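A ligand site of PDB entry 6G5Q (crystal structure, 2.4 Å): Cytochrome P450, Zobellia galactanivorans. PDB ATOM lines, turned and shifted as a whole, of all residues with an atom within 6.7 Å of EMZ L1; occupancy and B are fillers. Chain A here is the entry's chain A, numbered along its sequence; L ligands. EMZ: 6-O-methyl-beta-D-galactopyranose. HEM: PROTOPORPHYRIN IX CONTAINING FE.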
ATOM      1  N   GLY A  55      28.296  19.582   7.306  1.00  0.00           N
ATOM      2  CA  GLY A  55      29.656  20.113   7.507  1.00  0.00           C
ATOM      3  C   GLY A  55      30.726  19.048   7.686  1.00  0.00           C
ATOM      4  O   GLY A  55      31.909  19.365   7.638  1.00  0.00           O
ATOM      5  N   VAL A  58      33.170  18.336   4.506  1.00  0.00           N
ATOM      6  CA  VAL A  58      34.123  19.416   4.170  1.00  0.00           C
ATOM      7  C   VAL A  58      35.484  19.240   4.887  1.00  0.00           C
ATOM      8  O   VAL A  58      35.548  18.688   6.002  1.00  0.00           O
ATOM      9  CB  VAL A  58      33.515  20.814   4.431  1.00  0.00           C
ATOM     10  CG1 VAL A  58      34.461  21.926   3.958  1.00  0.00           C
ATOM     11  CG2 VAL A  58      32.157  20.937   3.722  1.00  0.00           C
ATOM     12  N   GLU A  62      33.314  21.373   9.070  1.00  0.00           N
ATOM     13  CA  GLU A  62      32.530  22.557   9.410  1.00  0.00           C
ATOM     14  C   GLU A  62      31.430  22.214  10.380  1.00  0.00           C
ATOM     15  O   GLU A  62      30.527  23.043  10.600  1.00  0.00           O
ATOM     16  CB  GLU A  62      31.931  23.215   8.151  1.00  0.00           C
ATOM     17  CG  GLU A  62      32.927  23.808   7.159  1.00  0.00           C
ATOM     18  CD  GLU A  62      32.308  24.370   5.869  1.00  0.00           C
ATOM     19  OE1 GLU A  62      31.107  24.131   5.559  1.00  0.00           O
ATOM     20  OE2 GLU A  62      33.056  25.061   5.154  1.00  0.00           O
ATOM     21  N   ARG A  66      28.298  25.240  11.442  1.00  0.00           N
ATOM     22  CA  ARG A  66      26.974  25.281  10.823  1.00  0.00           C
ATOM     23  C   ARG A  66      26.156  24.058  11.105  1.00  0.00           C
ATOM     24  O   ARG A  66      26.677  22.966  11.316  1.00  0.00           O
ATOM     25  CB  ARG A  66      27.046  25.573   9.299  1.00  0.00           C
ATOM     26  CG  ARG A  66      27.455  24.407   8.407  1.00  0.00           C
ATOM     27  CD  ARG A  66      27.435  24.811   6.920  1.00  0.00           C
ATOM     28  NE  ARG A  66      28.283  23.935   6.103  1.00  0.00           N
ATOM     29  CZ  ARG A  66      27.902  22.768   5.576  1.00  0.00           C
ATOM     30  NH1 ARG A  66      26.663  22.323   5.753  1.00  0.00           N
ATOM     31  NH2 ARG A  66      28.772  22.056   4.860  1.00  0.00           N
ATOM     32  N   GLN A  70      23.440  21.412   3.330  1.00  0.00           N
ATOM     33  CA  GLN A  70      23.554  22.004   2.002  1.00  0.00           C
ATOM     34  C   GLN A  70      22.941  21.078   0.962  1.00  0.00           C
ATOM     35  O   GLN A  70      23.020  19.838   1.098  1.00  0.00           O
ATOM     36  CB  GLN A  70      24.992  22.391   1.693  1.00  0.00           C
ATOM     37  CG  GLN A  70      25.416  23.599   2.524  1.00  0.00           C
ATOM     38  CD  GLN A  70      26.817  24.103   2.195  1.00  0.00           C
ATOM     39  OE1 GLN A  70      27.376  23.752   1.175  1.00  0.00           O
ATOM     40  NE2 GLN A  70      27.375  24.952   3.079  1.00  0.00           N
ATOM     41  N   PHE A  73      24.415  19.201  -2.290  1.00  0.00           N
ATOM     42  CA  PHE A  73      25.740  18.794  -1.833  1.00  0.00           C
ATOM     43  C   PHE A  73      25.803  17.723  -0.723  1.00  0.00           C
ATOM     44  O   PHE A  73      26.638  16.802  -0.780  1.00  0.00           O
ATOM     45  CB  PHE A  73      26.492  20.057  -1.397  1.00  0.00           C
ATOM     46  CG  PHE A  73      27.906  19.817  -0.915  1.00  0.00           C
ATOM     47  CD1 PHE A  73      28.845  19.137  -1.715  1.00  0.00           C
ATOM     48  CD2 PHE A  73      28.288  20.290   0.355  1.00  0.00           C
ATOM     49  CE1 PHE A  73      30.144  18.950  -1.248  1.00  0.00           C
ATOM     50  CE2 PHE A  73      29.583  20.098   0.815  1.00  0.00           C
ATOM     51  CZ  PHE A  73      30.503  19.426   0.005  1.00  0.00           C
ATOM     52  N   GLU A  74      24.917  17.820   0.272  1.00  0.00           N
ATOM     53  CA  GLU A  74      24.945  16.906   1.426  1.00  0.00           C
ATOM     54  C   GLU A  74      23.747  15.978   1.447  1.00  0.00           C
ATOM     55  O   GLU A  74      23.158  15.738   2.472  1.00  0.00           O
ATOM     56  CB  GLU A  74      25.101  17.686   2.753  1.00  0.00           C
ATOM     57  CG  GLU A  74      26.495  18.290   2.901  1.00  0.00           C
ATOM     58  CD  GLU A  74      26.648  19.313   4.012  1.00  0.00           C
ATOM     59  OE1 GLU A  74      25.676  20.065   4.295  1.00  0.00           O
ATOM     60  OE2 GLU A  74      27.789  19.406   4.558  1.00  0.00           O
ATOM     61  N   TYR A 173      25.185  33.404   6.712  1.00  0.00           N
ATOM     62  CA  TYR A 173      23.917  32.722   7.065  1.00  0.00           C
ATOM     63  C   TYR A 173      22.797  33.700   7.379  1.00  0.00           C
ATOM     64  O   TYR A 173      21.687  33.520   6.915  1.00  0.00           O
ATOM     65  CB  TYR A 173      24.052  31.698   8.197  1.00  0.00           C
ATOM     66  CG  TYR A 173      25.238  30.754   8.063  1.00  0.00           C
ATOM     67  CD1 TYR A 173      25.798  30.459   6.808  1.00  0.00           C
ATOM     68  CD2 TYR A 173      25.770  30.137   9.185  1.00  0.00           C
ATOM     69  CE1 TYR A 173      26.884  29.601   6.682  1.00  0.00           C
ATOM     70  CE2 TYR A 173      26.863  29.260   9.082  1.00  0.00           C
ATOM     71  CZ  TYR A 173      27.405  28.991   7.831  1.00  0.00           C
ATOM     72  OH  TYR A 173      28.473  28.117   7.725  1.00  0.00           O
ATOM     73  N   VAL A 215      23.230  28.802   0.578  1.00  0.00           N
ATOM     74  CA  VAL A 215      24.513  28.847   1.292  1.00  0.00           C
ATOM     75  C   VAL A 215      25.540  28.107   0.446  1.00  0.00           C
ATOM     76  O   VAL A 215      26.656  28.583   0.260  1.00  0.00           O
ATOM     77  CB  VAL A 215      24.429  28.273   2.738  1.00  0.00           C
ATOM     78  CG1 VAL A 215      25.812  28.182   3.386  1.00  0.00           C
ATOM     79  CG2 VAL A 215      23.522  29.152   3.598  1.00  0.00           C
ATOM     80  N   LEU A 216      25.127  26.975  -0.113  1.00  0.00           N
ATOM     81  CA  LEU A 216      25.969  26.223  -1.025  1.00  0.00           C
ATOM     82  C   LEU A 216      26.342  27.020  -2.272  1.00  0.00           C
ATOM     83  O   LEU A 216      27.457  26.938  -2.740  1.00  0.00           O
ATOM     84  CB  LEU A 216      25.293  24.906  -1.373  1.00  0.00           C
ATOM     85  CG  LEU A 216      25.883  24.097  -2.508  1.00  0.00           C
ATOM     86  CD1 LEU A 216      27.264  23.560  -2.165  1.00  0.00           C
ATOM     87  CD2 LEU A 216      24.895  22.991  -2.860  1.00  0.00           C
ATOM     88  N   THR A 217      25.396  27.808  -2.791  1.00  0.00           N
ATOM     89  CA  THR A 217      25.619  28.568  -4.014  1.00  0.00           C
ATOM     90  C   THR A 217      26.671  29.690  -3.825  1.00  0.00           C
ATOM     91  O   THR A 217      27.558  29.842  -4.685  1.00  0.00           O
ATOM     92  CB  THR A 217      24.309  29.091  -4.584  1.00  0.00           C
ATOM     93  OG1 THR A 217      23.460  27.975  -4.897  1.00  0.00           O
ATOM     94  CG2 THR A 217      24.536  29.922  -5.856  1.00  0.00           C
ATOM     95  N   PHE A 218      26.581  30.424  -2.692  1.00  0.00           N
ATOM     96  CA  PHE A 218      27.574  31.406  -2.325  1.00  0.00           C
ATOM     97  C   PHE A 218      28.921  30.822  -1.971  1.00  0.00           C
ATOM     98  O   PHE A 218      29.927  31.301  -2.469  1.00  0.00           O
ATOM     99  CB  PHE A 218      27.124  32.264  -1.152  1.00  0.00           C
ATOM    100  CG  PHE A 218      26.231  33.398  -1.537  1.00  0.00           C
ATOM    101  CD1 PHE A 218      24.866  33.193  -1.626  1.00  0.00           C
ATOM    102  CD2 PHE A 218      26.748  34.649  -1.771  1.00  0.00           C
ATOM    103  CE1 PHE A 218      24.000  34.246  -1.958  1.00  0.00           C
ATOM    104  CE2 PHE A 218      25.901  35.706  -2.115  1.00  0.00           C
ATOM    105  CZ  PHE A 218      24.527  35.507  -2.191  1.00  0.00           C
ATOM    106  N   ALA A 219      28.949  29.795  -1.123  1.00  0.00           N
ATOM    107  CA  ALA A 219      30.223  29.250  -0.664  1.00  0.00           C
ATOM    108  C   ALA A 219      30.966  28.392  -1.716  1.00  0.00           C
ATOM    109  O   ALA A 219      32.187  28.376  -1.744  1.00  0.00           O
ATOM    110  CB  ALA A 219      30.047  28.475   0.636  1.00  0.00           C
ATOM    111  N   GLY A 220      30.229  27.694  -2.580  1.00  0.00           N
ATOM    112  CA  GLY A 220      30.813  26.783  -3.552  1.00  0.00           C
ATOM    113  C   GLY A 220      31.574  27.461  -4.686  1.00  0.00           C
ATOM    114  O   GLY A 220      32.493  26.856  -5.304  1.00  0.00           O
ATOM    115  N   GLY A 221      31.218  28.699  -4.978  1.00  0.00           N
ATOM    116  CA  GLY A 221      31.769  29.344  -6.138  1.00  0.00           C
ATOM    117  C   GLY A 221      32.654  30.520  -5.871  1.00  0.00           C
ATOM    118  O   GLY A 221      33.117  31.146  -6.814  1.00  0.00           O
ATOM    119  N   ASP A 223      35.792  31.112  -3.556  1.00  0.00           N
ATOM    120  CA  ASP A 223      37.222  30.836  -3.585  1.00  0.00           C
ATOM    121  C   ASP A 223      37.701  30.156  -4.841  1.00  0.00           C
ATOM    122  O   ASP A 223      38.751  30.530  -5.398  1.00  0.00           O
ATOM    123  CB  ASP A 223      37.595  29.933  -2.410  1.00  0.00           C
ATOM    124  CG  ASP A 223      37.700  30.704  -1.089  1.00  0.00           C
ATOM    125  OD1 ASP A 223      37.522  31.958  -1.117  1.00  0.00           O
ATOM    126  OD2 ASP A 223      37.942  30.068  -0.038  1.00  0.00           O
ATOM    127  N   THR A 224      36.934  29.152  -5.273  1.00  0.00           N
ATOM    128  CA  THR A 224      37.255  28.426  -6.520  1.00  0.00           C
ATOM    129  C   THR A 224      37.357  29.380  -7.730  1.00  0.00           C
ATOM    130  O   THR A 224      38.334  29.353  -8.465  1.00  0.00           O
ATOM    131  CB  THR A 224      36.226  27.302  -6.799  1.00  0.00           C
ATOM    132  OG1 THR A 224      34.903  27.859  -6.779  1.00  0.00           O
ATOM    133  CG2 THR A 224      36.303  26.206  -5.758  1.00  0.00           C
ATOM    134  N   LEU A 267      39.507  23.438  -6.413  1.00  0.00           N
ATOM    135  CA  LEU A 267      39.006  22.732  -5.225  1.00  0.00           C
ATOM    136  C   LEU A 267      39.799  21.465  -5.079  1.00  0.00           C
ATOM    137  O   LEU A 267      39.650  20.505  -5.841  1.00  0.00           O
ATOM    138  CB  LEU A 267      37.498  22.408  -5.317  1.00  0.00           C
ATOM    139  CG  LEU A 267      36.743  21.724  -4.167  1.00  0.00           C
ATOM    140  CD1 LEU A 267      37.125  22.336  -2.833  1.00  0.00           C
ATOM    141  CD2 LEU A 267      35.255  21.902  -4.436  1.00  0.00           C
ATOM    142  N   MET A 270      37.543  16.898  -1.546  1.00  0.00           N
ATOM    143  CA  MET A 270      36.303  16.913  -0.823  1.00  0.00           C
ATOM    144  C   MET A 270      36.201  15.575  -0.117  1.00  0.00           C
ATOM    145  O   MET A 270      36.534  14.505  -0.677  1.00  0.00           O
ATOM    146  CB  MET A 270      35.127  17.077  -1.773  1.00  0.00           C
ATOM    147  CG  MET A 270      33.812  17.343  -1.074  1.00  0.00           C
ATOM    148  SD  MET A 270      33.981  18.607   0.209  1.00  0.00           S
ATOM    149  CE  MET A 270      34.162  20.106  -0.766  1.00  0.00           C
ATOM    150  N   HIS A 328      27.726  14.163  -7.909  1.00  0.00           N
ATOM    151  CA  HIS A 328      27.847  15.521  -7.401  1.00  0.00           C
ATOM    152  C   HIS A 328      28.630  16.478  -8.327  1.00  0.00           C
ATOM    153  O   HIS A 328      29.054  17.535  -7.881  1.00  0.00           O
ATOM    154  CB  HIS A 328      28.437  15.522  -5.975  1.00  0.00           C
ATOM    155  CG  HIS A 328      27.532  14.898  -4.958  1.00  0.00           C
ATOM    156  ND1 HIS A 328      26.504  15.606  -4.339  1.00  0.00           N
ATOM    157  CD2 HIS A 328      27.455  13.629  -4.470  1.00  0.00           C
ATOM    158  CE1 HIS A 328      25.838  14.797  -3.534  1.00  0.00           C
ATOM    159  NE2 HIS A 328      26.404  13.601  -3.580  1.00  0.00           N
HETATM  160  C4  EMZ L   1      30.409  23.839   0.779  1.00  0.00           C
HETATM  161  C5  EMZ L   1      31.424  23.414  -0.312  1.00  0.00           C
HETATM  162  C6  EMZ L   1      30.748  23.080  -1.627  1.00  0.00           C
HETATM  163  C3  EMZ L   1      31.175  24.353   1.990  1.00  0.00           C
HETATM  164  CAM EMZ L   1      31.160  21.765  -3.458  1.00  0.00           C
HETATM  165  O6  EMZ L   1      31.766  22.693  -2.561  1.00  0.00           O
HETATM  166  O5  EMZ L   1      32.350  24.481  -0.652  1.00  0.00           O
HETATM  167  C1  EMZ L   1      33.096  24.683   0.529  1.00  0.00           C
HETATM  168  O1  EMZ L   1      34.246  25.441   0.254  1.00  0.00           O
HETATM  169  C2  EMZ L   1      32.102  25.423   1.451  1.00  0.00           C
HETATM  170  O2  EMZ L   1      32.712  26.156   2.477  1.00  0.00           O
HETATM  171  O3  EMZ L   1      30.324  24.948   2.986  1.00  0.00           O
HETATM  172  O4  EMZ L   1      29.579  24.890   0.259  1.00  0.00           O
HETATM  173  CHA HEM L   2      30.255  20.792  -6.643  1.00  0.00           C
HETATM  174  CHB HEM L   2      34.531  22.488  -8.240  1.00  0.00           C
HETATM  175  CHC HEM L   2      32.555  26.762  -9.143  1.00  0.00           C
HETATM  176  CHD HEM L   2      28.482  25.239  -7.152  1.00  0.00           C
HETATM  177  C1A HEM L   2      31.589  20.891  -7.006  1.00  0.00           C
HETATM  178  C2A HEM L   2      32.550  19.844  -6.926  1.00  0.00           C
HETATM  179  C3A HEM L   2      33.728  20.349  -7.375  1.00  0.00           C
HETATM  180  C4A HEM L   2      33.530  21.681  -7.747  1.00  0.00           C
HETATM  181  CMA HEM L   2      35.031  19.615  -7.489  1.00  0.00           C
HETATM  182  CAA HEM L   2      32.393  18.402  -6.476  1.00  0.00           C
HETATM  183  CBA HEM L   2      32.016  18.368  -4.991  1.00  0.00           C
HETATM  184  CGA HEM L   2      31.826  16.976  -4.452  1.00  0.00           C
HETATM  185  O1A HEM L   2      31.324  16.854  -3.302  1.00  0.00           O
HETATM  186  O2A HEM L   2      32.140  15.956  -5.129  1.00  0.00           O
HETATM  187  C1B HEM L   2      34.328  23.798  -8.634  1.00  0.00           C
HETATM  188  C2B HEM L   2      35.345  24.545  -9.267  1.00  0.00           C
HETATM  189  C3B HEM L   2      34.818  25.768  -9.537  1.00  0.00           C
HETATM  190  C4B HEM L   2      33.419  25.706  -9.032  1.00  0.00           C
HETATM  191  CMB HEM L   2      36.742  24.062  -9.521  1.00  0.00           C
HETATM  192  CAB HEM L   2      35.474  26.985 -10.124  1.00  0.00           C
HETATM  193  CBB HEM L   2      36.349  26.977 -11.121  1.00  0.00           C
HETATM  194  C1C HEM L   2      31.264  26.735  -8.668  1.00  0.00           C
HETATM  195  C2C HEM L   2      30.378  27.835  -8.718  1.00  0.00           C
HETATM  196  C3C HEM L   2      29.211  27.408  -8.090  1.00  0.00           C
HETATM  197  C4C HEM L   2      29.424  26.033  -7.723  1.00  0.00           C
HETATM  198  CMC HEM L   2      30.704  29.213  -9.332  1.00  0.00           C
HETATM  199  CAC HEM L   2      27.943  28.130  -7.908  1.00  0.00           C
HETATM  200  CBC HEM L   2      27.794  29.412  -8.167  1.00  0.00           C
HETATM  201  C1D HEM L   2      28.627  23.864  -6.907  1.00  0.00           C
HETATM  202  C2D HEM L   2      27.499  23.042  -6.415  1.00  0.00           C
HETATM  203  C3D HEM L   2      27.990  21.792  -6.292  1.00  0.00           C
HETATM  204  C4D HEM L   2      29.420  21.889  -6.665  1.00  0.00           C
HETATM  205  CMD HEM L   2      26.080  23.494  -6.129  1.00  0.00           C
HETATM  206  CAD HEM L   2      27.195  20.597  -5.765  1.00  0.00           C
HETATM  207  CBD HEM L   2      26.562  19.769  -6.887  1.00  0.00           C
HETATM  208  CGD HEM L   2      25.838  18.568  -6.301  1.00  0.00           C
HETATM  209  O1D HEM L   2      26.095  18.209  -5.128  1.00  0.00           O
HETATM  210  O2D HEM L   2      24.996  17.889  -6.965  1.00  0.00           O
HETATM  211  NA  HEM L   2      32.234  22.009  -7.495  1.00  0.00           N
HETATM  212  NB  HEM L   2      33.192  24.501  -8.535  1.00  0.00           N
HETATM  213  NC  HEM L   2      30.685  25.688  -8.051  1.00  0.00           N
HETATM  214  ND  HEM L   2      29.728  23.150  -7.046  1.00  0.00           N
HETATM  215 FE   HEM L   2      31.381  23.778  -7.750  1.00  0.00          FE
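The side-chain amide nitrogen of Gln 70 lies close to the guanidinium group of Arg 66 (3.3 Å). OE1 of Glu 74 is in hydrogen-bond range of N of Gln 70 (2.8 Å). NE of Arg 66 lies within salt-bridge range of OE1 of Glu 62 (2.9 Å). N of Glu 62 lies within hydrogen-bond range of O of Gly 55 (2.8 Å). The side-chain carboxylate (OE2) of Glu 74 is in salt-bridge range of the guanidinium group (NH2) of Arg 66, 2.8 Å away.
Residues that only touch EMZ L1: Leu 216 (3.6 Å), Ala 219 (3.6 Å), Phe 73 (3.7 Å), Arg 66 (3.8 Å), Val 58 (3.95 Å) and Met 270 (3.96 Å). Hydrophobic or aromatic side chains within 4 Å of EMZ L1: Val 58, Phe 73, Leu 216, Ala 219 and Met 270. Within 4 Å of EMZ L1: Val 58, Glu 62, Arg 66, Gln 70, Phe 73, Leu 216, Ala 219 and Met 270. The nearest printed residue that does not touch EMZ L1 is Gly 220 (4.01 Å).
The side-chain amide oxygen (OE1) of Gln 70 sits at hydrogen-bond distance from an oxygen (O4) of EMZ L1, at 2.6 Å. The side-chain carboxylate (OE1) of Glu 62 is in hydrogen-bond range of an oxygen (O3) of EMZ L1 (2.8 Å). An oxygen (O1D) of HEM L2 sits close to the backbone NH (N) of Phe 73 (3.4 Å). ND1 of His 328 lies within hydrogen-bond range of O1D of HEM L2, 2.8 Å away.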
